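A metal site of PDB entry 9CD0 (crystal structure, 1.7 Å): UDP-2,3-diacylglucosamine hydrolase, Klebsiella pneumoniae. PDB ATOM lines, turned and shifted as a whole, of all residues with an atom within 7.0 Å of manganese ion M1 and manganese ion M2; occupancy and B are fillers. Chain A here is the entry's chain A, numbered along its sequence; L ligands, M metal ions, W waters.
ND2 of Asn 79 is in hydrogen-bond range of O3 of the ligand (2.9 Å).
The guanidinium group (NH1) of Arg 80 is in hydrogen-bond range of an oxygen (O5) of the ligand.
Of the 21 residues printed, 4 come within 4 Å of manganese ion M2.
Manganese ion M2 is bound by OD1 of Asp 8, water W1, NE2 of His 10, NE2 of His 197 and OD2 of Asp 41.
Manganese ion M2 has five donor atoms within binding distance.
Water W2 bridges an oxygen (O4) of the ligand and the side-chain amide nitrogen of Asn 79.
Of the 21 residues printed, 5 come within 4 Å of manganese ion M1.
Along chain A the residues within 4 Å of manganese ion M1 span positions 8 to 195.
A ring nitrogen (ND1) of His 114 lies within hydrogen-bond range of the backbone carbonyl oxygen of Leu 39 (2.7 Å).
N of Asp 8 sits at hydrogen-bond distance from O of Gly 40, at 3.0 Å.
The side-chain carboxylate (OD1) of Asp 41 sits at hydrogen-bond distance from the backbone NH (N) of Arg 80 (2.9 Å).
The side-chain carboxylate of Asp 8 lies within hydrogen-bond range of the backbone NH of His 195, 2.7 Å away.
O of Asp 41 sits at hydrogen-bond distance from N of Leu 9 (3.0 Å).
OE1 of Glu 44 sits at hydrogen-bond distance from ND1 of His 10 (2.8 Å).
The backbone NH (N) of Gly 194 lies within hydrogen-bond range of the backbone carbonyl oxygen (O) of His 114 (2.8 Å).
Manganese ion M1 is bound by water W1 (2.0 Å), OD1 of Asn 79 (2.0 Å), OD2 of Asp 41 (2.1 Å), NE2 of His 114 (2.2 Å) and ND1 of His 195 (2.2 Å).
Manganese ion M1 has five donor atoms within binding distance.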
ATOM      1  N   ALA A   7      15.762 -28.789  -7.388  1.00  0.00           N
ATOM      2  CA  ALA A   7      14.864 -28.180  -6.406  1.00  0.00           C
ATOM      3  C   ALA A   7      13.542 -27.868  -7.089  1.00  0.00           C
ATOM      4  O   ALA A   7      13.429 -27.879  -8.326  1.00  0.00           O
ATOM      5  CB  ALA A   7      15.475 -26.906  -5.782  1.00  0.00           C
ATOM      6  N   ASP A   8      12.507 -27.569  -6.272  1.00  0.00           N
ATOM      7  CA  ASP A   8      11.298 -27.032  -6.810  1.00  0.00           C
ATOM      8  C   ASP A   8      10.651 -27.944  -7.863  1.00  0.00           C
ATOM      9  O   ASP A   8      10.064 -27.472  -8.849  1.00  0.00           O
ATOM     10  CB  ASP A   8      11.588 -25.640  -7.367  1.00  0.00           C
ATOM     11  CG  ASP A   8      12.090 -24.721  -6.238  1.00  0.00           C
ATOM     12  OD1 ASP A   8      11.280 -24.500  -5.342  1.00  0.00           O
ATOM     13  OD2 ASP A   8      13.268 -24.305  -6.227  1.00  0.00           O
ATOM     14  N   LEU A   9      10.639 -29.209  -7.574  1.00  0.00           N
ATOM     15  CA  LEU A   9       9.863 -30.161  -8.376  1.00  0.00           C
ATOM     16  C   LEU A   9       8.381 -30.057  -8.047  1.00  0.00           C
ATOM     17  O   LEU A   9       7.541 -30.195  -8.953  1.00  0.00           O
ATOM     18  CB  LEU A   9      10.336 -31.579  -8.089  1.00  0.00           C
ATOM     19  CG  LEU A   9      11.713 -31.907  -8.725  1.00  0.00           C
ATOM     20  CD1 LEU A   9      12.876 -31.464  -7.776  1.00  0.00           C
ATOM     21  CD2 LEU A   9      11.776 -33.432  -9.034  1.00  0.00           C
ATOM     22  N   HIS A  10       8.042 -29.708  -6.813  1.00  0.00           N
ATOM     23  CA  HIS A  10       6.648 -29.527  -6.386  1.00  0.00           C
ATOM     24  C   HIS A  10       5.799 -30.735  -6.791  1.00  0.00           C
ATOM     25  O   HIS A  10       4.711 -30.600  -7.375  1.00  0.00           O
ATOM     26  CB  HIS A  10       6.058 -28.200  -6.952  1.00  0.00           C
ATOM     27  CG  HIS A  10       6.653 -26.950  -6.349  1.00  0.00           C
ATOM     28  ND1 HIS A  10       6.069 -26.278  -5.293  1.00  0.00           N
ATOM     29  CD2 HIS A  10       7.837 -26.336  -6.568  1.00  0.00           C
ATOM     30  CE1 HIS A  10       6.834 -25.246  -4.959  1.00  0.00           C
ATOM     31  NE2 HIS A  10       7.904 -25.256  -5.723  1.00  0.00           N
ATOM     32  N   LEU A  39      17.389 -29.403  -3.095  1.00  0.00           N
ATOM     33  CA  LEU A  39      17.376 -28.172  -2.288  1.00  0.00           C
ATOM     34  C   LEU A  39      15.957 -27.671  -2.007  1.00  0.00           C
ATOM     35  O   LEU A  39      15.682 -26.471  -2.147  1.00  0.00           O
ATOM     36  CB  LEU A  39      18.199 -27.078  -2.991  1.00  0.00           C
ATOM     37  CG  LEU A  39      19.656 -27.503  -3.249  1.00  0.00           C
ATOM     38  CD1 LEU A  39      20.482 -26.254  -3.760  1.00  0.00           C
ATOM     39  CD2 LEU A  39      20.372 -28.134  -1.991  1.00  0.00           C
ATOM     40  N   GLY A  40      15.069 -28.557  -1.557  1.00  0.00           N
ATOM     41  CA  GLY A  40      13.761 -28.080  -1.078  1.00  0.00           C
ATOM     42  C   GLY A  40      12.661 -28.078  -2.134  1.00  0.00           C
ATOM     43  O   GLY A  40      12.900 -28.013  -3.328  1.00  0.00           O
ATOM     44  N   ASP A  41      11.403 -28.109  -1.652  1.00  0.00           N
ATOM     45  CA  ASP A  41      10.218 -28.165  -2.515  1.00  0.00           C
ATOM     46  C   ASP A  41      10.292 -29.357  -3.481  1.00  0.00           C
ATOM     47  O   ASP A  41       9.941 -29.273  -4.671  1.00  0.00           O
ATOM     48  CB  ASP A  41       9.977 -26.839  -3.270  1.00  0.00           C
ATOM     49  CG  ASP A  41       9.610 -25.684  -2.335  1.00  0.00           C
ATOM     50  OD1 ASP A  41       9.472 -25.905  -1.093  1.00  0.00           O
ATOM     51  OD2 ASP A  41       9.500 -24.582  -2.900  1.00  0.00           O
ATOM     52  N   GLU A  44       4.950 -30.708  -3.447  1.00  0.00           N
ATOM     53  CA  GLU A  44       4.063 -29.559  -3.360  1.00  0.00           C
ATOM     54  C   GLU A  44       3.521 -29.343  -1.942  1.00  0.00           C
ATOM     55  O   GLU A  44       3.193 -28.209  -1.564  1.00  0.00           O
ATOM     56  CB  GLU A  44       2.901 -29.751  -4.349  1.00  0.00           C
ATOM     57  CG  GLU A  44       1.808 -28.626  -4.248  1.00  0.00           C
ATOM     58  CD  GLU A  44       2.237 -27.236  -4.632  1.00  0.00           C
ATOM     59  OE1 GLU A  44       3.360 -27.040  -5.122  1.00  0.00           O
ATOM     60  OE2 GLU A  44       1.421 -26.314  -4.462  1.00  0.00           O
ATOM     61  N   GLY A  78      12.264 -27.221   1.826  1.00  0.00           N
ATOM     62  CA  GLY A  78      11.688 -26.027   1.219  1.00  0.00           C
ATOM     63  C   GLY A  78      10.576 -25.440   2.092  1.00  0.00           C
ATOM     64  O   GLY A  78      10.261 -25.926   3.156  1.00  0.00           O
ATOM     65  N   ASN A  79       9.966 -24.355   1.593  1.00  0.00           N
ATOM     66  CA  ASN A  79       8.780 -23.820   2.275  1.00  0.00           C
ATOM     67  C   ASN A  79       7.565 -24.733   2.127  1.00  0.00           C
ATOM     68  O   ASN A  79       6.636 -24.642   2.945  1.00  0.00           O
ATOM     69  CB  ASN A  79       8.498 -22.413   1.746  1.00  0.00           C
ATOM     70  CG  ASN A  79       8.207 -22.391   0.260  1.00  0.00           C
ATOM     71  OD1 ASN A  79       9.094 -22.635  -0.513  1.00  0.00           O
ATOM     72  ND2 ASN A  79       6.987 -22.068  -0.120  1.00  0.00           N
ATOM     73  N   ARG A  80       7.530 -25.569   1.089  1.00  0.00           N
ATOM     74  CA  ARG A  80       6.384 -26.465   0.935  1.00  0.00           C
ATOM     75  C   ARG A  80       6.527 -27.703   1.831  1.00  0.00           C
ATOM     76  O   ARG A  80       5.526 -28.151   2.418  1.00  0.00           O
ATOM     77  CB  ARG A  80       6.178 -26.904  -0.520  1.00  0.00           C
ATOM     78  CG  ARG A  80       6.068 -25.747  -1.494  1.00  0.00           C
ATOM     79  CD  ARG A  80       4.920 -24.803  -1.127  1.00  0.00           C
ATOM     80  NE  ARG A  80       3.634 -25.495  -1.151  1.00  0.00           N
ATOM     81  CZ  ARG A  80       2.451 -24.885  -1.206  1.00  0.00           C
ATOM     82  NH1 ARG A  80       2.328 -23.574  -1.149  1.00  0.00           N
ATOM     83  NH2 ARG A  80       1.347 -25.622  -1.328  1.00  0.00           N
ATOM     84  N   HIS A 114      17.618 -23.583   0.412  1.00  0.00           N
ATOM     85  CA  HIS A 114      16.442 -23.538  -0.462  1.00  0.00           C
ATOM     86  C   HIS A 114      16.322 -22.162  -1.127  1.00  0.00           C
ATOM     87  O   HIS A 114      16.000 -22.083  -2.314  1.00  0.00           O
ATOM     88  CB  HIS A 114      15.139 -23.840   0.305  1.00  0.00           C
ATOM     89  CG  HIS A 114      13.937 -23.808  -0.571  1.00  0.00           C
ATOM     90  ND1 HIS A 114      13.771 -24.643  -1.659  1.00  0.00           N
ATOM     91  CD2 HIS A 114      12.840 -23.009  -0.519  1.00  0.00           C
ATOM     92  CE1 HIS A 114      12.590 -24.358  -2.232  1.00  0.00           C
ATOM     93  NE2 HIS A 114      12.020 -23.366  -1.561  1.00  0.00           N
ATOM     94  N   GLY A 115      16.548 -21.087  -0.357  1.00  0.00           N
ATOM     95  CA  GLY A 115      16.579 -19.709  -0.821  1.00  0.00           C
ATOM     96  C   GLY A 115      15.447 -18.864  -0.283  1.00  0.00           C
ATOM     97  O   GLY A 115      15.490 -17.626  -0.425  1.00  0.00           O
ATOM     98  N   ASP A 116      14.434 -19.472   0.339  1.00  0.00           N
ATOM     99  CA  ASP A 116      13.349 -18.633   0.853  1.00  0.00           C
ATOM    100  C   ASP A 116      13.836 -17.696   1.966  1.00  0.00           C
ATOM    101  O   ASP A 116      13.269 -16.593   2.140  1.00  0.00           O
ATOM    102  CB  ASP A 116      12.183 -19.487   1.393  1.00  0.00           C
ATOM    103  CG  ASP A 116      12.619 -20.467   2.451  1.00  0.00           C
ATOM    104  OD1 ASP A 116      13.565 -21.216   2.202  1.00  0.00           O
ATOM    105  OD2 ASP A 116      12.069 -20.443   3.571  1.00  0.00           O
ATOM    106  N   TYR A 125       5.421 -13.805   4.135  1.00  0.00           N
ATOM    107  CA  TYR A 125       6.000 -15.151   4.080  1.00  0.00           C
ATOM    108  C   TYR A 125       6.863 -15.403   5.314  1.00  0.00           C
ATOM    109  O   TYR A 125       6.809 -16.473   5.902  1.00  0.00           O
ATOM    110  CB  TYR A 125       6.856 -15.350   2.796  1.00  0.00           C
ATOM    111  CG  TYR A 125       7.599 -16.643   2.950  1.00  0.00           C
ATOM    112  CD1 TYR A 125       6.896 -17.810   3.079  1.00  0.00           C
ATOM    113  CD2 TYR A 125       8.987 -16.675   3.149  1.00  0.00           C
ATOM    114  CE1 TYR A 125       7.514 -19.032   3.322  1.00  0.00           C
ATOM    115  CE2 TYR A 125       9.647 -17.882   3.382  1.00  0.00           C
ATOM    116  CZ  TYR A 125       8.885 -19.059   3.469  1.00  0.00           C
ATOM    117  OH  TYR A 125       9.465 -20.274   3.729  1.00  0.00           O
ATOM    118  N   ILE A 171       6.052 -15.677  -6.480  1.00  0.00           N
ATOM    119  CA  ILE A 171       7.019 -15.835  -5.396  1.00  0.00           C
ATOM    120  C   ILE A 171       7.942 -14.634  -5.410  1.00  0.00           C
ATOM    121  O   ILE A 171       8.463 -14.254  -6.467  1.00  0.00           O
ATOM    122  CB  ILE A 171       7.819 -17.141  -5.556  1.00  0.00           C
ATOM    123  CG1 ILE A 171       6.859 -18.359  -5.588  1.00  0.00           C
ATOM    124  CG2 ILE A 171       8.945 -17.245  -4.556  1.00  0.00           C
ATOM    125  CD1 ILE A 171       7.510 -19.633  -6.073  1.00  0.00           C
ATOM    126  N   GLY A 194      17.219 -22.572  -4.733  1.00  0.00           N
ATOM    127  CA  GLY A 194      16.046 -22.565  -5.576  1.00  0.00           C
ATOM    128  C   GLY A 194      15.040 -21.584  -5.045  1.00  0.00           C
ATOM    129  O   GLY A 194      15.357 -20.394  -4.869  1.00  0.00           O
ATOM    130  N   HIS A 195      13.801 -22.072  -4.803  1.00  0.00           N
ATOM    131  CA  HIS A 195      12.685 -21.267  -4.298  1.00  0.00           C
ATOM    132  C   HIS A 195      12.108 -20.194  -5.220  1.00  0.00           C
ATOM    133  O   HIS A 195      10.881 -20.129  -5.360  1.00  0.00           O
ATOM    134  CB  HIS A 195      13.042 -20.615  -2.958  1.00  0.00           C
ATOM    135  CG  HIS A 195      11.878 -19.869  -2.341  1.00  0.00           C
ATOM    136  ND1 HIS A 195      10.753 -20.522  -1.892  1.00  0.00           N
ATOM    137  CD2 HIS A 195      11.627 -18.546  -2.170  1.00  0.00           C
ATOM    138  CE1 HIS A 195       9.876 -19.641  -1.435  1.00  0.00           C
ATOM    139  NE2 HIS A 195      10.389 -18.437  -1.573  1.00  0.00           N
ATOM    140  N   THR A 196      12.941 -19.314  -5.833  1.00  0.00           N
ATOM    141  CA  THR A 196      12.369 -18.199  -6.586  1.00  0.00           C
ATOM    142  C   THR A 196      11.918 -18.564  -7.985  1.00  0.00           C
ATOM    143  O   THR A 196      11.233 -17.737  -8.615  1.00  0.00           O
ATOM    144  CB  THR A 196      13.389 -17.063  -6.692  1.00  0.00           C
ATOM    145  OG1 THR A 196      14.524 -17.537  -7.432  1.00  0.00           O
ATOM    146  CG2 THR A 196      13.867 -16.685  -5.290  1.00  0.00           C
ATOM    147  N   HIS A 197      12.283 -19.782  -8.483  1.00  0.00           N
ATOM    148  CA  HIS A 197      11.780 -20.287  -9.768  1.00  0.00           C
ATOM    149  C   HIS A 197      12.262 -19.403 -10.926  1.00  0.00           C
ATOM    150  O   HIS A 197      11.566 -19.228 -11.945  1.00  0.00           O
ATOM    151  CB  HIS A 197      10.246 -20.402  -9.762  1.00  0.00           C
ATOM    152  CG  HIS A 197       9.702 -21.403  -8.755  1.00  0.00           C
ATOM    153  ND1 HIS A 197       8.356 -21.744  -8.695  1.00  0.00           N
ATOM    154  CD2 HIS A 197      10.319 -22.137  -7.802  1.00  0.00           C
ATOM    155  CE1 HIS A 197       8.179 -22.623  -7.717  1.00  0.00           C
ATOM    156  NE2 HIS A 197       9.350 -22.870  -7.169  1.00  0.00           N
ATOM    157  N   ALA A 218      12.132 -24.320 -11.353  1.00  0.00           N
ATOM    158  CA  ALA A 218      11.024 -25.212 -11.048  1.00  0.00           C
ATOM    159  C   ALA A 218      10.773 -26.182 -12.189  1.00  0.00           C
ATOM    160  O   ALA A 218      11.020 -25.904 -13.372  1.00  0.00           O
ATOM    161  CB  ALA A 218       9.719 -24.434 -10.762  1.00  0.00           C
HETATM  162  C1  LIG L   1      -0.413 -27.183   6.610  1.00  0.00           C
HETATM  163  C2  LIG L   1       0.747 -24.942   2.461  1.00  0.00           C
HETATM  164  C3  LIG L   1       2.443 -23.245   2.267  1.00  0.00           C
HETATM  165  C4  LIG L   1       3.753 -21.126   1.824  1.00  0.00           C
HETATM  166  C5  LIG L   1       3.096 -19.017   2.929  1.00  0.00           C
HETATM  167  C6  LIG L   1       3.404 -16.884   1.904  1.00  0.00           C
HETATM  168  C7  LIG L   1       4.096 -18.853   0.710  1.00  0.00           C
HETATM  169  C8  LIG L   1       2.202 -26.484  10.613  1.00  0.00           C
HETATM  170  C9  LIG L   1       0.890 -26.698   8.768  1.00  0.00           C
HETATM  171  C10 LIG L   1       1.954 -27.957   6.919  1.00  0.00           C
HETATM  172  C11 LIG L   1       2.237 -27.487   5.495  1.00  0.00           C
HETATM  173  C12 LIG L   1      -0.059 -26.714   5.194  1.00  0.00           C
HETATM  174  C13 LIG L   1       1.784 -25.841   2.692  1.00  0.00           C
HETATM  175  C14 LIG L   1       1.100 -23.609   2.264  1.00  0.00           C
HETATM  176  C15 LIG L   1       3.508 -24.127   2.550  1.00  0.00           C
HETATM  177  C16 LIG L   1       3.140 -25.461   2.760  1.00  0.00           C
HETATM  178  C17 LIG L   1       3.640 -19.629   1.766  1.00  0.00           C
HETATM  179  C18 LIG L   1       2.969 -17.625   2.989  1.00  0.00           C
HETATM  180  C19 LIG L   1       3.952 -17.494   0.777  1.00  0.00           C
HETATM  181  C20 LIG L   1       2.943 -18.707  -2.610  1.00  0.00           C
HETATM  182  C21 LIG L   1       5.986 -18.879  -0.937  1.00  0.00           C
HETATM  183  C22 LIG L   1       1.176 -21.233   2.198  1.00  0.00           C
HETATM  184  C23 LIG L   1       0.261 -22.389   1.939  1.00  0.00           C
HETATM  185  C24 LIG L   1      -0.224 -26.039   9.360  1.00  0.00           C
HETATM  186  C25 LIG L   1      -0.021 -25.642  10.630  1.00  0.00           C
HETATM  187  C26 LIG L   1       1.184 -25.817  11.308  1.00  0.00           C
HETATM  188  C27 LIG L   1      -1.179 -24.909  11.349  1.00  0.00           C
HETATM  189  F1  LIG L   1      -2.293 -25.464  11.088  1.00  0.00           F
HETATM  190  F2  LIG L   1      -0.939 -24.852  12.605  1.00  0.00           F
HETATM  191  F3  LIG L   1      -1.280 -23.758  10.910  1.00  0.00           F
HETATM  192  N1  LIG L   1       2.012 -26.916   9.402  1.00  0.00           N
HETATM  193  N2  LIG L   1       0.796 -27.186   7.450  1.00  0.00           N
HETATM  194  N3  LIG L   1       1.057 -27.579   4.699  1.00  0.00           N
HETATM  195  N4  LIG L   1       2.511 -21.806   2.061  1.00  0.00           N
HETATM  196  N5  LIG L   1       4.669 -19.374  -0.490  1.00  0.00           N
HETATM  197  O1  LIG L   1       0.082 -27.710   2.403  1.00  0.00           O
HETATM  198  O2  LIG L   1       2.308 -28.418   2.750  1.00  0.00           O
HETATM  199  O3  LIG L   1       4.809 -21.671   1.712  1.00  0.00           O
HETATM  200  O4  LIG L   1       4.355 -21.016  -2.403  1.00  0.00           O
HETATM  201  O5  LIG L   1       2.525 -20.709  -0.912  1.00  0.00           O
HETATM  202  S1  LIG L   1       1.260 -27.518   3.030  1.00  0.00           S
HETATM  203  S2  LIG L   1       3.630 -20.043  -1.591  1.00  0.00           S
HETATM  204 CL1  LIG L   1       3.750 -26.792  11.399  1.00  0.00          CL
HETATM  205 MN    MN M   1      10.101 -22.642  -2.245  1.00  0.00          MN
HETATM  206 MN    MN M   2       9.392 -23.853  -5.213  1.00  0.00          MN
HETATM  207  O   HOH W   1       9.290 -22.255  -4.007  1.00  0.00           O
HETATM  208  O   HOH W   2       6.818 -22.196  -3.124  1.00  0.00           O
